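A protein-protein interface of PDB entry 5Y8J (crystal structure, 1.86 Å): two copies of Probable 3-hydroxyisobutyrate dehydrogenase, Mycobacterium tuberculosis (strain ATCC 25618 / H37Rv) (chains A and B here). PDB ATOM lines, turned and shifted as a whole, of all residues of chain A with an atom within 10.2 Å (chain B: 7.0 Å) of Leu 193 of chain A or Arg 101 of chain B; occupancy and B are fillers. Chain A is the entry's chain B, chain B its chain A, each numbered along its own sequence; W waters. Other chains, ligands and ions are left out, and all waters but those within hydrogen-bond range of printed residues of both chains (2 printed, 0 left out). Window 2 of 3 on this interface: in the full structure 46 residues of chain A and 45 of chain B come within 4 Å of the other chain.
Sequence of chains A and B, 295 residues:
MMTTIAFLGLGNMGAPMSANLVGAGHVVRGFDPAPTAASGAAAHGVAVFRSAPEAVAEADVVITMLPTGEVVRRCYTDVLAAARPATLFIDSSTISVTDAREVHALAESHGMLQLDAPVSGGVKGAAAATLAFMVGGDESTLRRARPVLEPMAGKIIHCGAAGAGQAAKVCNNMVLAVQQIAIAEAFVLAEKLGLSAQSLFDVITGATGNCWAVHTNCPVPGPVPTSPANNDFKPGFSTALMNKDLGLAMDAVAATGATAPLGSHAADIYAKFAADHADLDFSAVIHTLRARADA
The side-chain sulfur (SG) of Cys 171 of chain B lies within hydrogen-bond range of the backbone carbonyl oxygen (O) of Ala 186 of chain A. NH2 of Arg 101 of chain B lies within hydrogen-bond range of O of Leu 193 of chain A.
No position is printed for both chains.
Of the printed residues of chain B, Leu 189 of chain A touches Ala 252 (3.9 Å) and Thr 256 (3.6 Å). Of the printed residues of chain B, Lys 192 of chain A touches Thr 256. Leu 193 of chain A touches three residues of chain B. Of the printed residues of chain B, Leu 195 of chain A touches Ala 164 (3.99 Å), Ala 167 (3.9 Å) and Ala 168 (3.6 Å). No residue of chain A comes within 4 Å of Val 97 of chain B. Arg 101 of chain B touches just one residue of chain A: Leu 193 (2.7 Å). Ala 161 of chain B touches none of the printed residues of chain A. Ala 162 of chain B touches none of the printed residues of chain A. No residue of chain A comes within 4 Å of Gly 163 of chain B. Printed residues of chain A within 4 Å of Ala 164 of chain B: Leu 195 (3.99 Å). Of chain A, only Leu 193 (3.9 Å) and Leu 195 (3.9 Å) come within 4 Å of Ala 167 of chain B. Of chain A, only Leu 189 comes within 4 Å of Ala 252 of chain B. Printed residues of chain A within 4 Å of Thr 256 of chain B: Leu 189 (3.6 Å), Lys 192 (3.6 Å) and Leu 193 (3.6 Å).
Water W2 lies within hydrogen-bond range of O of Lys 192 of chain A (2.8 Å), O of Leu 193 of chain A (3.3 Å) and NH1 of Arg 101 of chain B (3.3 Å). Water W1 bridges O of Gly 194 of chain A (3.1 Å) and N of Ala 161 of chain B (3.1 Å).
Of the 14 printed residues of chain A, 6 touch a printed residue of chain B. Of the 29 printed residues of chain B, 7 touch a printed residue of chain A. Along chain B the printed residues that touch a printed residue of chain A span positions 101 to 256. Among the printed residues, 11 pairs touch across the chains. Among the printed residues, no Asp or Glu carboxylate lies within 4 Å of a Lys or Arg side-chain nitrogen of the other chain.
Among the printed residues, merely in contact across the chains: Leu 195 of chain A with Ala 168 of chain B (3.6 Å), Leu 189 of chain A with Thr 256 of chain B (3.6 Å), Leu 200 of chain A with Cys 171 of chain B (3.6 Å), Leu 193 of chain A with Thr 256 of chain B (3.6 Å), Lys 192 of chain A with Thr 256 of chain B (3.6 Å), Leu 195 of chain A with Ala 167 of chain B (3.9 Å), Leu 189 of chain A with Ala 252 of chain B (3.9 Å), Leu 193 of chain A with Ala 167 of chain B (3.9 Å) and Leu 195 of chain A with Ala 164 of chain B (3.99 Å).
N of Leu 195 of chain A lies within hydrogen-bond range of O of Ala 190 of chain A. NE of Arg 101 of chain B lies within hydrogen-bond range of O of Ala 162 of chain B. The side-chain sulfur of Cys 171 of chain B lies within hydrogen-bond range of the backbone carbonyl oxygen of Ala 167 of chain B, 3.3 Å away. The backbone carbonyl oxygen (O) of Val 253 of chain B lies within hydrogen-bond range of the side-chain hydroxyl (OG1) of Thr 256 of chain B (3.3 Å). O of Ala 252 of chain B lies within hydrogen-bond range of OG1 of Thr 256 of chain B.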
ATOM      1  N   GLU A 185      12.798   0.307   5.749  1.00  0.00           N
ATOM      2  CA  GLU A 185      12.906  -0.288   4.436  1.00  0.00           C
ATOM      3  C   GLU A 185      14.202  -1.094   4.278  1.00  0.00           C
ATOM      4  O   GLU A 185      14.150  -2.228   3.720  1.00  0.00           O
ATOM      5  CB  GLU A 185      12.884   0.778   3.355  1.00  0.00           C
ATOM      6  CG  GLU A 185      11.626   1.637   3.265  1.00  0.00           C
ATOM      7  CD  GLU A 185      11.701   2.708   2.179  1.00  0.00           C
ATOM      8  OE1 GLU A 185      12.759   2.832   1.451  1.00  0.00           O
ATOM      9  OE2 GLU A 185      10.665   3.459   2.074  1.00  0.00           O
ATOM     10  N   ALA A 186      15.337  -0.556   4.760  1.00  0.00           N
ATOM     11  CA  ALA A 186      16.592  -1.299   4.659  1.00  0.00           C
ATOM     12  C   ALA A 186      16.505  -2.606   5.455  1.00  0.00           C
ATOM     13  O   ALA A 186      16.952  -3.627   4.967  1.00  0.00           O
ATOM     14  CB  ALA A 186      17.728  -0.444   5.155  1.00  0.00           C
ATOM     15  N   PHE A 187      15.969  -2.595   6.709  1.00  0.00           N
ATOM     16  CA  PHE A 187      15.881  -3.821   7.484  1.00  0.00           C
ATOM     17  C   PHE A 187      14.956  -4.881   6.870  1.00  0.00           C
ATOM     18  O   PHE A 187      15.292  -6.069   6.943  1.00  0.00           O
ATOM     19  CB  PHE A 187      15.480  -3.557   8.974  1.00  0.00           C
ATOM     20  CG  PHE A 187      16.620  -3.160   9.826  1.00  0.00           C
ATOM     21  CD1 PHE A 187      17.486  -4.138  10.307  1.00  0.00           C
ATOM     22  CD2 PHE A 187      16.868  -1.861  10.111  1.00  0.00           C
ATOM     23  CE1 PHE A 187      18.573  -3.801  11.115  1.00  0.00           C
ATOM     24  CE2 PHE A 187      17.947  -1.500  10.878  1.00  0.00           C
ATOM     25  CZ  PHE A 187      18.822  -2.493  11.383  1.00  0.00           C
ATOM     26  N   VAL A 188      13.839  -4.494   6.243  1.00  0.00           N
ATOM     27  CA  VAL A 188      12.957  -5.474   5.668  1.00  0.00           C
ATOM     28  C   VAL A 188      13.573  -6.003   4.369  1.00  0.00           C
ATOM     29  O   VAL A 188      13.466  -7.197   4.100  1.00  0.00           O
ATOM     30  CB  VAL A 188      11.543  -4.902   5.457  1.00  0.00           C
ATOM     31  CG1 VAL A 188      10.663  -5.975   4.881  1.00  0.00           C
ATOM     32  CG2 VAL A 188      10.912  -4.482   6.803  1.00  0.00           C
ATOM     33  N   LEU A 189      14.247  -5.137   3.603  1.00  0.00           N
ATOM     34  CA  LEU A 189      14.979  -5.594   2.413  1.00  0.00           C
ATOM     35  C   LEU A 189      16.080  -6.587   2.780  1.00  0.00           C
ATOM     36  O   LEU A 189      16.224  -7.639   2.124  1.00  0.00           O
ATOM     37  CB  LEU A 189      15.511  -4.400   1.602  1.00  0.00           C
ATOM     38  CG  LEU A 189      16.278  -4.800   0.320  1.00  0.00           C
ATOM     39  CD1 LEU A 189      15.457  -5.597  -0.713  1.00  0.00           C
ATOM     40  CD2 LEU A 189      16.834  -3.563  -0.364  1.00  0.00           C
ATOM     41  N   ALA A 190      16.809  -6.285   3.861  1.00  0.00           N
ATOM     42  CA  ALA A 190      17.866  -7.163   4.341  1.00  0.00           C
ATOM     43  C   ALA A 190      17.265  -8.510   4.618  1.00  0.00           C
ATOM     44  O   ALA A 190      17.823  -9.519   4.216  1.00  0.00           O
ATOM     45  CB  ALA A 190      18.537  -6.633   5.613  1.00  0.00           C
ATOM     46  N   GLU A 191      16.160  -8.531   5.335  1.00  0.00           N
ATOM     47  CA  GLU A 191      15.494  -9.768   5.693  1.00  0.00           C
ATOM     48  C   GLU A 191      15.147 -10.600   4.479  1.00  0.00           C
ATOM     49  O   GLU A 191      15.318 -11.824   4.501  1.00  0.00           O
ATOM     50  CB  GLU A 191      14.211  -9.549   6.497  1.00  0.00           C
ATOM     51  CG  GLU A 191      13.623 -10.871   7.016  1.00  0.00           C
ATOM     52  CD  GLU A 191      12.232 -11.260   6.445  1.00  0.00           C
ATOM     53  OE1 GLU A 191      11.242 -10.549   6.836  1.00  0.00           O
ATOM     54  OE2 GLU A 191      12.079 -12.285   5.674  1.00  0.00           O
ATOM     55  N   LYS A 192      14.605  -9.963   3.460  1.00  0.00           N
ATOM     56  CA  LYS A 192      14.219 -10.681   2.264  1.00  0.00           C
ATOM     57  C   LYS A 192      15.430 -11.170   1.477  1.00  0.00           C
ATOM     58  O   LYS A 192      15.333 -12.167   0.767  1.00  0.00           O
ATOM     59  CB  LYS A 192      13.367  -9.827   1.360  1.00  0.00           C
ATOM     60  CG  LYS A 192      11.970  -9.562   1.992  1.00  0.00           C
ATOM     61  CD  LYS A 192      11.143  -8.695   1.080  1.00  0.00           C
ATOM     62  CE  LYS A 192       9.632  -8.940   1.275  1.00  0.00           C
ATOM     63  NZ  LYS A 192       9.078  -8.076   2.346  1.00  0.00           N
ATOM     64  N   LEU A 193      16.526 -10.429   1.550  1.00  0.00           N
ATOM     65  CA  LEU A 193      17.777 -10.854   0.961  1.00  0.00           C
ATOM     66  C   LEU A 193      18.557 -11.933   1.722  1.00  0.00           C
ATOM     67  O   LEU A 193      19.626 -12.359   1.225  1.00  0.00           O
ATOM     68  CB  LEU A 193      18.683  -9.627   0.746  1.00  0.00           C
ATOM     69  CG  LEU A 193      18.241  -8.630  -0.323  1.00  0.00           C
ATOM     70  CD1 LEU A 193      19.071  -7.340  -0.305  1.00  0.00           C
ATOM     71  CD2 LEU A 193      18.120  -9.190  -1.730  1.00  0.00           C
ATOM     72  N   GLY A 194      18.113 -12.278   2.915  1.00  0.00           N
ATOM     73  CA  GLY A 194      18.819 -13.163   3.857  1.00  0.00           C
ATOM     74  C   GLY A 194      19.996 -12.568   4.600  1.00  0.00           C
ATOM     75  O   GLY A 194      20.856 -13.287   5.063  1.00  0.00           O
ATOM     76  N   LEU A 195      20.072 -11.242   4.671  1.00  0.00           N
ATOM     77  CA  LEU A 195      21.072 -10.572   5.481  1.00  0.00           C
ATOM     78  C   LEU A 195      20.505 -10.400   6.950  1.00  0.00           C
ATOM     79  O   LEU A 195      19.430  -9.820   7.112  1.00  0.00           O
ATOM     80  CB  LEU A 195      21.441  -9.228   4.815  1.00  0.00           C
ATOM     81  CG  LEU A 195      22.284  -8.226   5.648  1.00  0.00           C
ATOM     82  CD1 LEU A 195      23.657  -8.790   5.898  1.00  0.00           C
ATOM     83  CD2 LEU A 195      22.401  -6.934   4.878  1.00  0.00           C
ATOM     84  N   SER A 196      21.220 -10.872   7.988  1.00  0.00           N
ATOM     85  CA  SER A 196      20.662 -10.761   9.383  1.00  0.00           C
ATOM     86  C   SER A 196      20.489  -9.311   9.836  1.00  0.00           C
ATOM     87  O   SER A 196      21.201  -8.391   9.369  1.00  0.00           O
ATOM     88  CB  SER A 196      21.459 -11.526  10.455  1.00  0.00           C
ATOM     89  OG  SER A 196      22.669 -10.906  10.725  1.00  0.00           O
ATOM     90  N   ALA A 197      19.492  -9.114  10.702  1.00  0.00           N
ATOM     91  CA  ALA A 197      19.269  -7.819  11.278  1.00  0.00           C
ATOM     92  C   ALA A 197      20.501  -7.372  12.007  1.00  0.00           C
ATOM     93  O   ALA A 197      20.904  -6.190  11.930  1.00  0.00           O
ATOM     94  CB  ALA A 197      18.088  -7.905  12.262  1.00  0.00           C
ATOM     95  N   LEU A 200      23.175  -6.201   9.377  1.00  0.00           N
ATOM     96  CA  LEU A 200      22.828  -4.932   8.768  1.00  0.00           C
ATOM     97  C   LEU A 200      23.039  -3.806   9.786  1.00  0.00           C
ATOM     98  O   LEU A 200      23.584  -2.778   9.462  1.00  0.00           O
ATOM     99  CB  LEU A 200      21.389  -4.909   8.260  1.00  0.00           C
ATOM    100  CG  LEU A 200      21.046  -3.551   7.641  1.00  0.00           C
ATOM    101  CD1 LEU A 200      21.752  -3.299   6.353  1.00  0.00           C
ATOM    102  CD2 LEU A 200      19.534  -3.353   7.363  1.00  0.00           C
ATOM    103  N   ILE B  95      27.886  -5.719  -7.565  1.00  0.00           N
ATOM    104  CA  ILE B  95      26.913  -6.379  -8.420  1.00  0.00           C
ATOM    105  C   ILE B  95      25.724  -6.797  -7.591  1.00  0.00           C
ATOM    106  O   ILE B  95      25.749  -6.734  -6.355  1.00  0.00           O
ATOM    107  CB  ILE B  95      27.521  -7.540  -9.199  1.00  0.00           C
ATOM    108  CG1 ILE B  95      27.969  -8.699  -8.233  1.00  0.00           C
ATOM    109  CG2 ILE B  95      28.703  -7.050 -10.052  1.00  0.00           C
ATOM    110  CD1 ILE B  95      28.569  -9.885  -8.972  1.00  0.00           C
ATOM    111  N   SER B  96      24.656  -7.216  -8.272  1.00  0.00           N
ATOM    112  CA  SER B  96      23.516  -7.686  -7.512  1.00  0.00           C
ATOM    113  C   SER B  96      23.809  -8.866  -6.615  1.00  0.00           C
ATOM    114  O   SER B  96      24.677  -9.707  -6.861  1.00  0.00           O
ATOM    115  CB  SER B  96      22.305  -8.026  -8.384  1.00  0.00           C
ATOM    116  OG  SER B  96      22.570  -9.234  -9.144  1.00  0.00           O
ATOM    117  N   VAL B  97      22.963  -8.991  -5.602  1.00  0.00           N
ATOM    118  CA  VAL B  97      23.032 -10.103  -4.643  1.00  0.00           C
ATOM    119  C   VAL B  97      22.826 -11.417  -5.373  1.00  0.00           C
ATOM    120  O   VAL B  97      23.509 -12.403  -5.087  1.00  0.00           O
ATOM    121  CB  VAL B  97      22.019  -9.893  -3.453  1.00  0.00           C
ATOM    122  CG1 VAL B  97      21.933 -11.077  -2.509  1.00  0.00           C
ATOM    123  CG2 VAL B  97      22.329  -8.630  -2.667  1.00  0.00           C
ATOM    124  N   THR B  98      21.815 -11.471  -6.264  1.00  0.00           N
ATOM    125  CA  THR B  98      21.592 -12.665  -7.117  1.00  0.00           C
ATOM    126  C   THR B  98      22.796 -13.075  -7.913  1.00  0.00           C
ATOM    127  O   THR B  98      23.197 -14.241  -7.895  1.00  0.00           O
ATOM    128  CB  THR B  98      20.423 -12.398  -8.086  1.00  0.00           C
ATOM    129  OG1 THR B  98      19.278 -12.096  -7.269  1.00  0.00           O
ATOM    130  CG2 THR B  98      20.098 -13.661  -8.868  1.00  0.00           C
ATOM    131  N   ASP B  99      23.373 -12.114  -8.614  1.00  0.00           N
ATOM    132  CA  ASP B  99      24.638 -12.348  -9.385  1.00  0.00           C
ATOM    133  C   ASP B  99      25.816 -12.813  -8.522  1.00  0.00           C
ATOM    134  O   ASP B  99      26.454 -13.841  -8.844  1.00  0.00           O
ATOM    135  CB  ASP B  99      25.041 -11.094 -10.204  1.00  0.00           C
ATOM    136  CG  ASP B  99      24.103 -10.858 -11.421  1.00  0.00           C
ATOM    137  OD1 ASP B  99      23.326 -11.748 -11.812  1.00  0.00           O
ATOM    138  OD2 ASP B  99      24.193  -9.803 -12.020  1.00  0.00           O
ATOM    139  N   ALA B 100      26.015 -12.134  -7.375  1.00  0.00           N
ATOM    140  CA  ALA B 100      26.967 -12.610  -6.426  1.00  0.00           C
ATOM    141  C   ALA B 100      26.838 -14.047  -5.956  1.00  0.00           C
ATOM    142  O   ALA B 100      27.803 -14.824  -5.956  1.00  0.00           O
ATOM    143  CB  ALA B 100      26.983 -11.667  -5.230  1.00  0.00           C
ATOM    144  N   ARG B 101      25.648 -14.425  -5.562  1.00  0.00           N
ATOM    145  CA  ARG B 101      25.367 -15.800  -5.179  1.00  0.00           C
ATOM    146  C   ARG B 101      25.567 -16.786  -6.293  1.00  0.00           C
ATOM    147  O   ARG B 101      26.086 -17.907  -6.048  1.00  0.00           O
ATOM    148  CB  ARG B 101      23.960 -15.913  -4.557  1.00  0.00           C
ATOM    149  CG  ARG B 101      23.949 -15.213  -3.190  1.00  0.00           C
ATOM    150  CD  ARG B 101      22.583 -15.244  -2.527  1.00  0.00           C
ATOM    151  NE  ARG B 101      22.715 -14.652  -1.203  1.00  0.00           N
ATOM    152  CZ  ARG B 101      21.732 -14.090  -0.505  1.00  0.00           C
ATOM    153  NH1 ARG B 101      20.513 -13.965  -1.039  1.00  0.00           N
ATOM    154  NH2 ARG B 101      22.015 -13.583   0.693  1.00  0.00           N
ATOM    155  N   GLU B 102      25.210 -16.400  -7.501  1.00  0.00           N
ATOM    156  CA  GLU B 102      25.416 -17.289  -8.628  1.00  0.00           C
ATOM    157  C   GLU B 102      26.903 -17.526  -8.884  1.00  0.00           C
ATOM    158  O   GLU B 102      27.326 -18.686  -9.097  1.00  0.00           O
ATOM    159  CB  GLU B 102      24.755 -16.777  -9.874  1.00  0.00           C
ATOM    160  CG  GLU B 102      25.042 -17.586 -11.147  1.00  0.00           C
ATOM    161  CD  GLU B 102      24.407 -16.960 -12.415  1.00  0.00           C
ATOM    162  OE1 GLU B 102      23.385 -16.245 -12.304  1.00  0.00           O
ATOM    163  OE2 GLU B 102      24.924 -17.193 -13.529  1.00  0.00           O
ATOM    164  N   VAL B 103      27.708 -16.457  -8.896  1.00  0.00           N
ATOM    165  CA  VAL B 103      29.119 -16.670  -9.147  1.00  0.00           C
ATOM    166  C   VAL B 103      29.848 -17.345  -7.988  1.00  0.00           C
ATOM    167  O   VAL B 103      30.836 -18.029  -8.211  1.00  0.00           O
ATOM    168  CB  VAL B 103      29.876 -15.411  -9.595  1.00  0.00           C
ATOM    169  CG1 VAL B 103      29.273 -14.832 -10.878  1.00  0.00           C
ATOM    170  CG2 VAL B 103      29.903 -14.345  -8.524  1.00  0.00           C
ATOM    171  N   HIS B 104      29.377 -17.135  -6.749  1.00  0.00           N
ATOM    172  CA  HIS B 104      29.929 -17.817  -5.622  1.00  0.00           C
ATOM    173  C   HIS B 104      29.748 -19.334  -5.838  1.00  0.00           C
ATOM    174  O   HIS B 104      30.707 -20.135  -5.674  1.00  0.00           O
ATOM    175  CB  HIS B 104      29.204 -17.391  -4.365  1.00  0.00           C
ATOM    176  CG  HIS B 104      29.564 -18.195  -3.180  1.00  0.00           C
ATOM    177  ND1 HIS B 104      30.730 -17.982  -2.467  1.00  0.00           N
ATOM    178  CD2 HIS B 104      28.919 -19.201  -2.563  1.00  0.00           C
ATOM    179  CE1 HIS B 104      30.787 -18.850  -1.475  1.00  0.00           C
ATOM    180  NE2 HIS B 104      29.706 -19.590  -1.514  1.00  0.00           N
ATOM    181  N   ALA B 105      28.528 -19.732  -6.135  1.00  0.00           N
ATOM    182  CA  ALA B 105      28.219 -21.170  -6.313  1.00  0.00           C
ATOM    183  C   ALA B 105      29.010 -21.749  -7.477  1.00  0.00           C
ATOM    184  O   ALA B 105      29.473 -22.904  -7.423  1.00  0.00           O
ATOM    185  CB  ALA B 105      26.729 -21.361  -6.575  1.00  0.00           C
ATOM    186  N   LEU B 106      29.165 -20.979  -8.534  1.00  0.00           N
ATOM    187  CA  LEU B 106      29.986 -21.454  -9.669  1.00  0.00           C
ATOM    188  C   LEU B 106      31.449 -21.749  -9.307  1.00  0.00           C
ATOM    189  O   LEU B 106      32.017 -22.792  -9.587  1.00  0.00           O
ATOM    190  CB  LEU B 106      29.908 -20.402 -10.748  1.00  0.00           C
ATOM    191  CG  LEU B 106      30.711 -20.558 -12.002  1.00  0.00           C
ATOM    192  CD1 LEU B 106      30.248 -21.783 -12.766  1.00  0.00           C
ATOM    193  CD2 LEU B 106      30.510 -19.279 -12.834  1.00  0.00           C
ATOM    194  N   GLN B 114      35.357 -18.855  -2.314  1.00  0.00           N
ATOM    195  CA  GLN B 114      34.936 -17.565  -2.900  1.00  0.00           C
ATOM    196  C   GLN B 114      34.265 -16.689  -1.912  1.00  0.00           C
ATOM    197  O   GLN B 114      33.426 -17.145  -1.126  1.00  0.00           O
ATOM    198  CB  GLN B 114      34.082 -17.807  -4.141  1.00  0.00           C
ATOM    199  CG  GLN B 114      33.917 -16.647  -5.070  1.00  0.00           C
ATOM    200  CD  GLN B 114      32.786 -15.701  -4.670  1.00  0.00           C
ATOM    201  OE1 GLN B 114      32.024 -15.876  -3.696  1.00  0.00           O
ATOM    202  NE2 GLN B 114      32.636 -14.716  -5.508  1.00  0.00           N
ATOM    203  N   ASP B 116      32.311 -12.627  -1.774  1.00  0.00           N
ATOM    204  CA  ASP B 116      31.957 -11.278  -2.254  1.00  0.00           C
ATOM    205  C   ASP B 116      32.493 -10.274  -1.228  1.00  0.00           C
ATOM    206  O   ASP B 116      32.318 -10.448  -0.013  1.00  0.00           O
ATOM    207  CB  ASP B 116      30.418 -11.058  -2.470  1.00  0.00           C
ATOM    208  CG  ASP B 116      29.547 -11.403  -1.286  1.00  0.00           C
ATOM    209  OD1 ASP B 116      29.585 -12.590  -0.874  1.00  0.00           O
ATOM    210  OD2 ASP B 116      28.711 -10.521  -0.807  1.00  0.00           O
ATOM    211  N   ALA B 161      26.717 -14.960   5.026  1.00  0.00           N
ATOM    212  CA  ALA B 161      26.986 -15.980   3.962  1.00  0.00           C
ATOM    213  C   ALA B 161      27.089 -15.279   2.589  1.00  0.00           C
ATOM    214  O   ALA B 161      26.837 -14.056   2.442  1.00  0.00           O
ATOM    215  CB  ALA B 161      25.901 -17.068   3.984  1.00  0.00           C
ATOM    216  N   ALA B 162      27.474 -16.029   1.567  1.00  0.00           N
ATOM    217  CA  ALA B 162      27.694 -15.458   0.246  1.00  0.00           C
ATOM    218  C   ALA B 162      26.489 -14.562  -0.180  1.00  0.00           C
ATOM    219  O   ALA B 162      25.311 -14.920  -0.014  1.00  0.00           O
ATOM    220  CB  ALA B 162      27.883 -16.587  -0.801  1.00  0.00           C
ATOM    221  N   GLY B 163      26.827 -13.430  -0.693  1.00  0.00           N
ATOM    222  CA  GLY B 163      25.952 -12.349  -1.081  1.00  0.00           C
ATOM    223  C   GLY B 163      25.614 -11.284  -0.009  1.00  0.00           C
ATOM    224  O   GLY B 163      25.075 -10.184  -0.317  1.00  0.00           O
ATOM    225  N   ALA B 164      25.954 -11.560   1.242  1.00  0.00           N
ATOM    226  CA  ALA B 164      25.675 -10.631   2.328  1.00  0.00           C
ATOM    227  C   ALA B 164      26.477  -9.335   2.239  1.00  0.00           C
ATOM    228  O   ALA B 164      26.036  -8.294   2.728  1.00  0.00           O
ATOM    229  CB  ALA B 164      25.939 -11.299   3.674  1.00  0.00           C
ATOM    230  N   GLN B 166      27.340  -7.770  -0.642  1.00  0.00           N
ATOM    231  CA  GLN B 166      26.582  -6.976  -1.583  1.00  0.00           C
ATOM    232  C   GLN B 166      25.305  -6.423  -0.937  1.00  0.00           C
ATOM    233  O   GLN B 166      24.962  -5.254  -1.116  1.00  0.00           O
ATOM    234  CB  GLN B 166      26.248  -7.762  -2.850  1.00  0.00           C
ATOM    235  CG  GLN B 166      27.425  -8.326  -3.660  1.00  0.00           C
ATOM    236  CD  GLN B 166      28.328  -7.269  -4.306  1.00  0.00           C
ATOM    237  OE1 GLN B 166      28.057  -6.070  -4.298  1.00  0.00           O
ATOM    238  NE2 GLN B 166      29.447  -7.727  -4.850  1.00  0.00           N
ATOM    239  N   ALA B 167      24.621  -7.279  -0.222  1.00  0.00           N
ATOM    240  CA  ALA B 167      23.318  -6.867   0.378  1.00  0.00           C
ATOM    241  C   ALA B 167      23.546  -5.751   1.371  1.00  0.00           C
ATOM    242  O   ALA B 167      22.779  -4.789   1.407  1.00  0.00           O
ATOM    243  CB  ALA B 167      22.696  -8.012   1.062  1.00  0.00           C
ATOM    244  N   ALA B 168      24.551  -5.919   2.238  1.00  0.00           N
ATOM    245  CA  ALA B 168      24.841  -4.866   3.242  1.00  0.00           C
ATOM    246  C   ALA B 168      25.199  -3.518   2.589  1.00  0.00           C
ATOM    247  O   ALA B 168      24.694  -2.421   2.989  1.00  0.00           O
ATOM    248  CB  ALA B 168      25.960  -5.309   4.183  1.00  0.00           C
ATOM    249  N   VAL B 170      24.338  -2.440  -0.494  1.00  0.00           N
ATOM    250  CA  VAL B 170      23.266  -1.861  -1.237  1.00  0.00           C
ATOM    251  C   VAL B 170      22.233  -1.257  -0.250  1.00  0.00           C
ATOM    252  O   VAL B 170      21.650  -0.193  -0.488  1.00  0.00           O
ATOM    253  CB  VAL B 170      22.699  -2.880  -2.259  1.00  0.00           C
ATOM    254  CG1 VAL B 170      21.763  -3.942  -1.641  1.00  0.00           C
ATOM    255  CG2 VAL B 170      22.040  -2.168  -3.406  1.00  0.00           C
ATOM    256  N   CYS B 171      22.022  -1.945   0.855  1.00  0.00           N
ATOM    257  CA  CYS B 171      21.083  -1.437   1.882  1.00  0.00           C
ATOM    258  C   CYS B 171      21.599  -0.168   2.521  1.00  0.00           C
ATOM    259  O   CYS B 171      20.867   0.849   2.610  1.00  0.00           O
ATOM    260  CB  CYS B 171      20.782  -2.491   2.965  1.00  0.00           C
ATOM    261  SG  CYS B 171      19.757  -3.850   2.426  1.00  0.00           S
ATOM    262  N   ALA B 249      19.960  -1.497  -5.900  1.00  0.00           N
ATOM    263  CA  ALA B 249      18.945  -1.573  -4.884  1.00  0.00           C
ATOM    264  C   ALA B 249      17.576  -1.859  -5.496  1.00  0.00           C
ATOM    265  O   ALA B 249      16.819  -2.646  -4.905  1.00  0.00           O
ATOM    266  CB  ALA B 249      18.884  -0.276  -4.076  1.00  0.00           C
ATOM    267  N   ASP B 251      16.938  -3.407  -8.299  1.00  0.00           N
ATOM    268  CA  ASP B 251      16.974  -4.830  -8.667  1.00  0.00           C
ATOM    269  C   ASP B 251      16.699  -5.739  -7.473  1.00  0.00           C
ATOM    270  O   ASP B 251      16.027  -6.736  -7.590  1.00  0.00           O
ATOM    271  CB  ASP B 251      18.354  -5.225  -9.161  1.00  0.00           C
ATOM    272  CG  ASP B 251      18.747  -4.569 -10.476  1.00  0.00           C
ATOM    273  OD1 ASP B 251      17.872  -4.163 -11.225  1.00  0.00           O
ATOM    274  OD2 ASP B 251      20.008  -4.439 -10.773  1.00  0.00           O
ATOM    275  N   ALA B 252      17.287  -5.460  -6.334  1.00  0.00           N
ATOM    276  CA  ALA B 252      17.100  -6.268  -5.201  1.00  0.00           C
ATOM    277  C   ALA B 252      15.615  -6.161  -4.720  1.00  0.00           C
ATOM    278  O   ALA B 252      15.013  -7.168  -4.287  1.00  0.00           O
ATOM    279  CB  ALA B 252      18.046  -5.860  -4.110  1.00  0.00           C
ATOM    280  N   VAL B 253      15.064  -4.947  -4.811  1.00  0.00           N
ATOM    281  CA  VAL B 253      13.668  -4.705  -4.382  1.00  0.00           C
ATOM    282  C   VAL B 253      12.731  -5.515  -5.329  1.00  0.00           C
ATOM    283  O   VAL B 253      11.801  -6.176  -4.861  1.00  0.00           O
ATOM    284  CB  VAL B 253      13.404  -3.230  -4.401  1.00  0.00           C
ATOM    285  CG1 VAL B 253      11.893  -2.898  -4.332  1.00  0.00           C
ATOM    286  CG2 VAL B 253      14.138  -2.555  -3.218  1.00  0.00           C
ATOM    287  N   ALA B 255      13.601  -8.189  -7.175  1.00  0.00           N
ATOM    288  CA  ALA B 255      13.828  -9.624  -7.042  1.00  0.00           C
ATOM    289  C   ALA B 255      13.096 -10.177  -5.794  1.00  0.00           C
ATOM    290  O   ALA B 255      12.728 -11.350  -5.744  1.00  0.00           O
ATOM    291  CB  ALA B 255      15.329  -9.925  -6.954  1.00  0.00           C
ATOM    292  N   THR B 256      12.981  -9.373  -4.751  1.00  0.00           N
ATOM    293  CA  THR B 256      12.401  -9.866  -3.467  1.00  0.00           C
ATOM    294  C   THR B 256      10.925  -9.549  -3.261  1.00  0.00           C
ATOM    295  O   THR B 256      10.309 -10.058  -2.318  1.00  0.00           O
ATOM    296  CB  THR B 256      13.133  -9.307  -2.241  1.00  0.00           C
ATOM    297  OG1 THR B 256      13.158  -7.878  -2.318  1.00  0.00           O
ATOM    298  CG2 THR B 256      14.584  -9.825  -2.226  1.00  0.00           C
HETATM  299  O   HOH W   1      23.788 -14.057   5.487  1.00  0.00           O
HETATM  300  O   HOH W   2      17.272 -13.786  -0.527  1.00  0.00           O
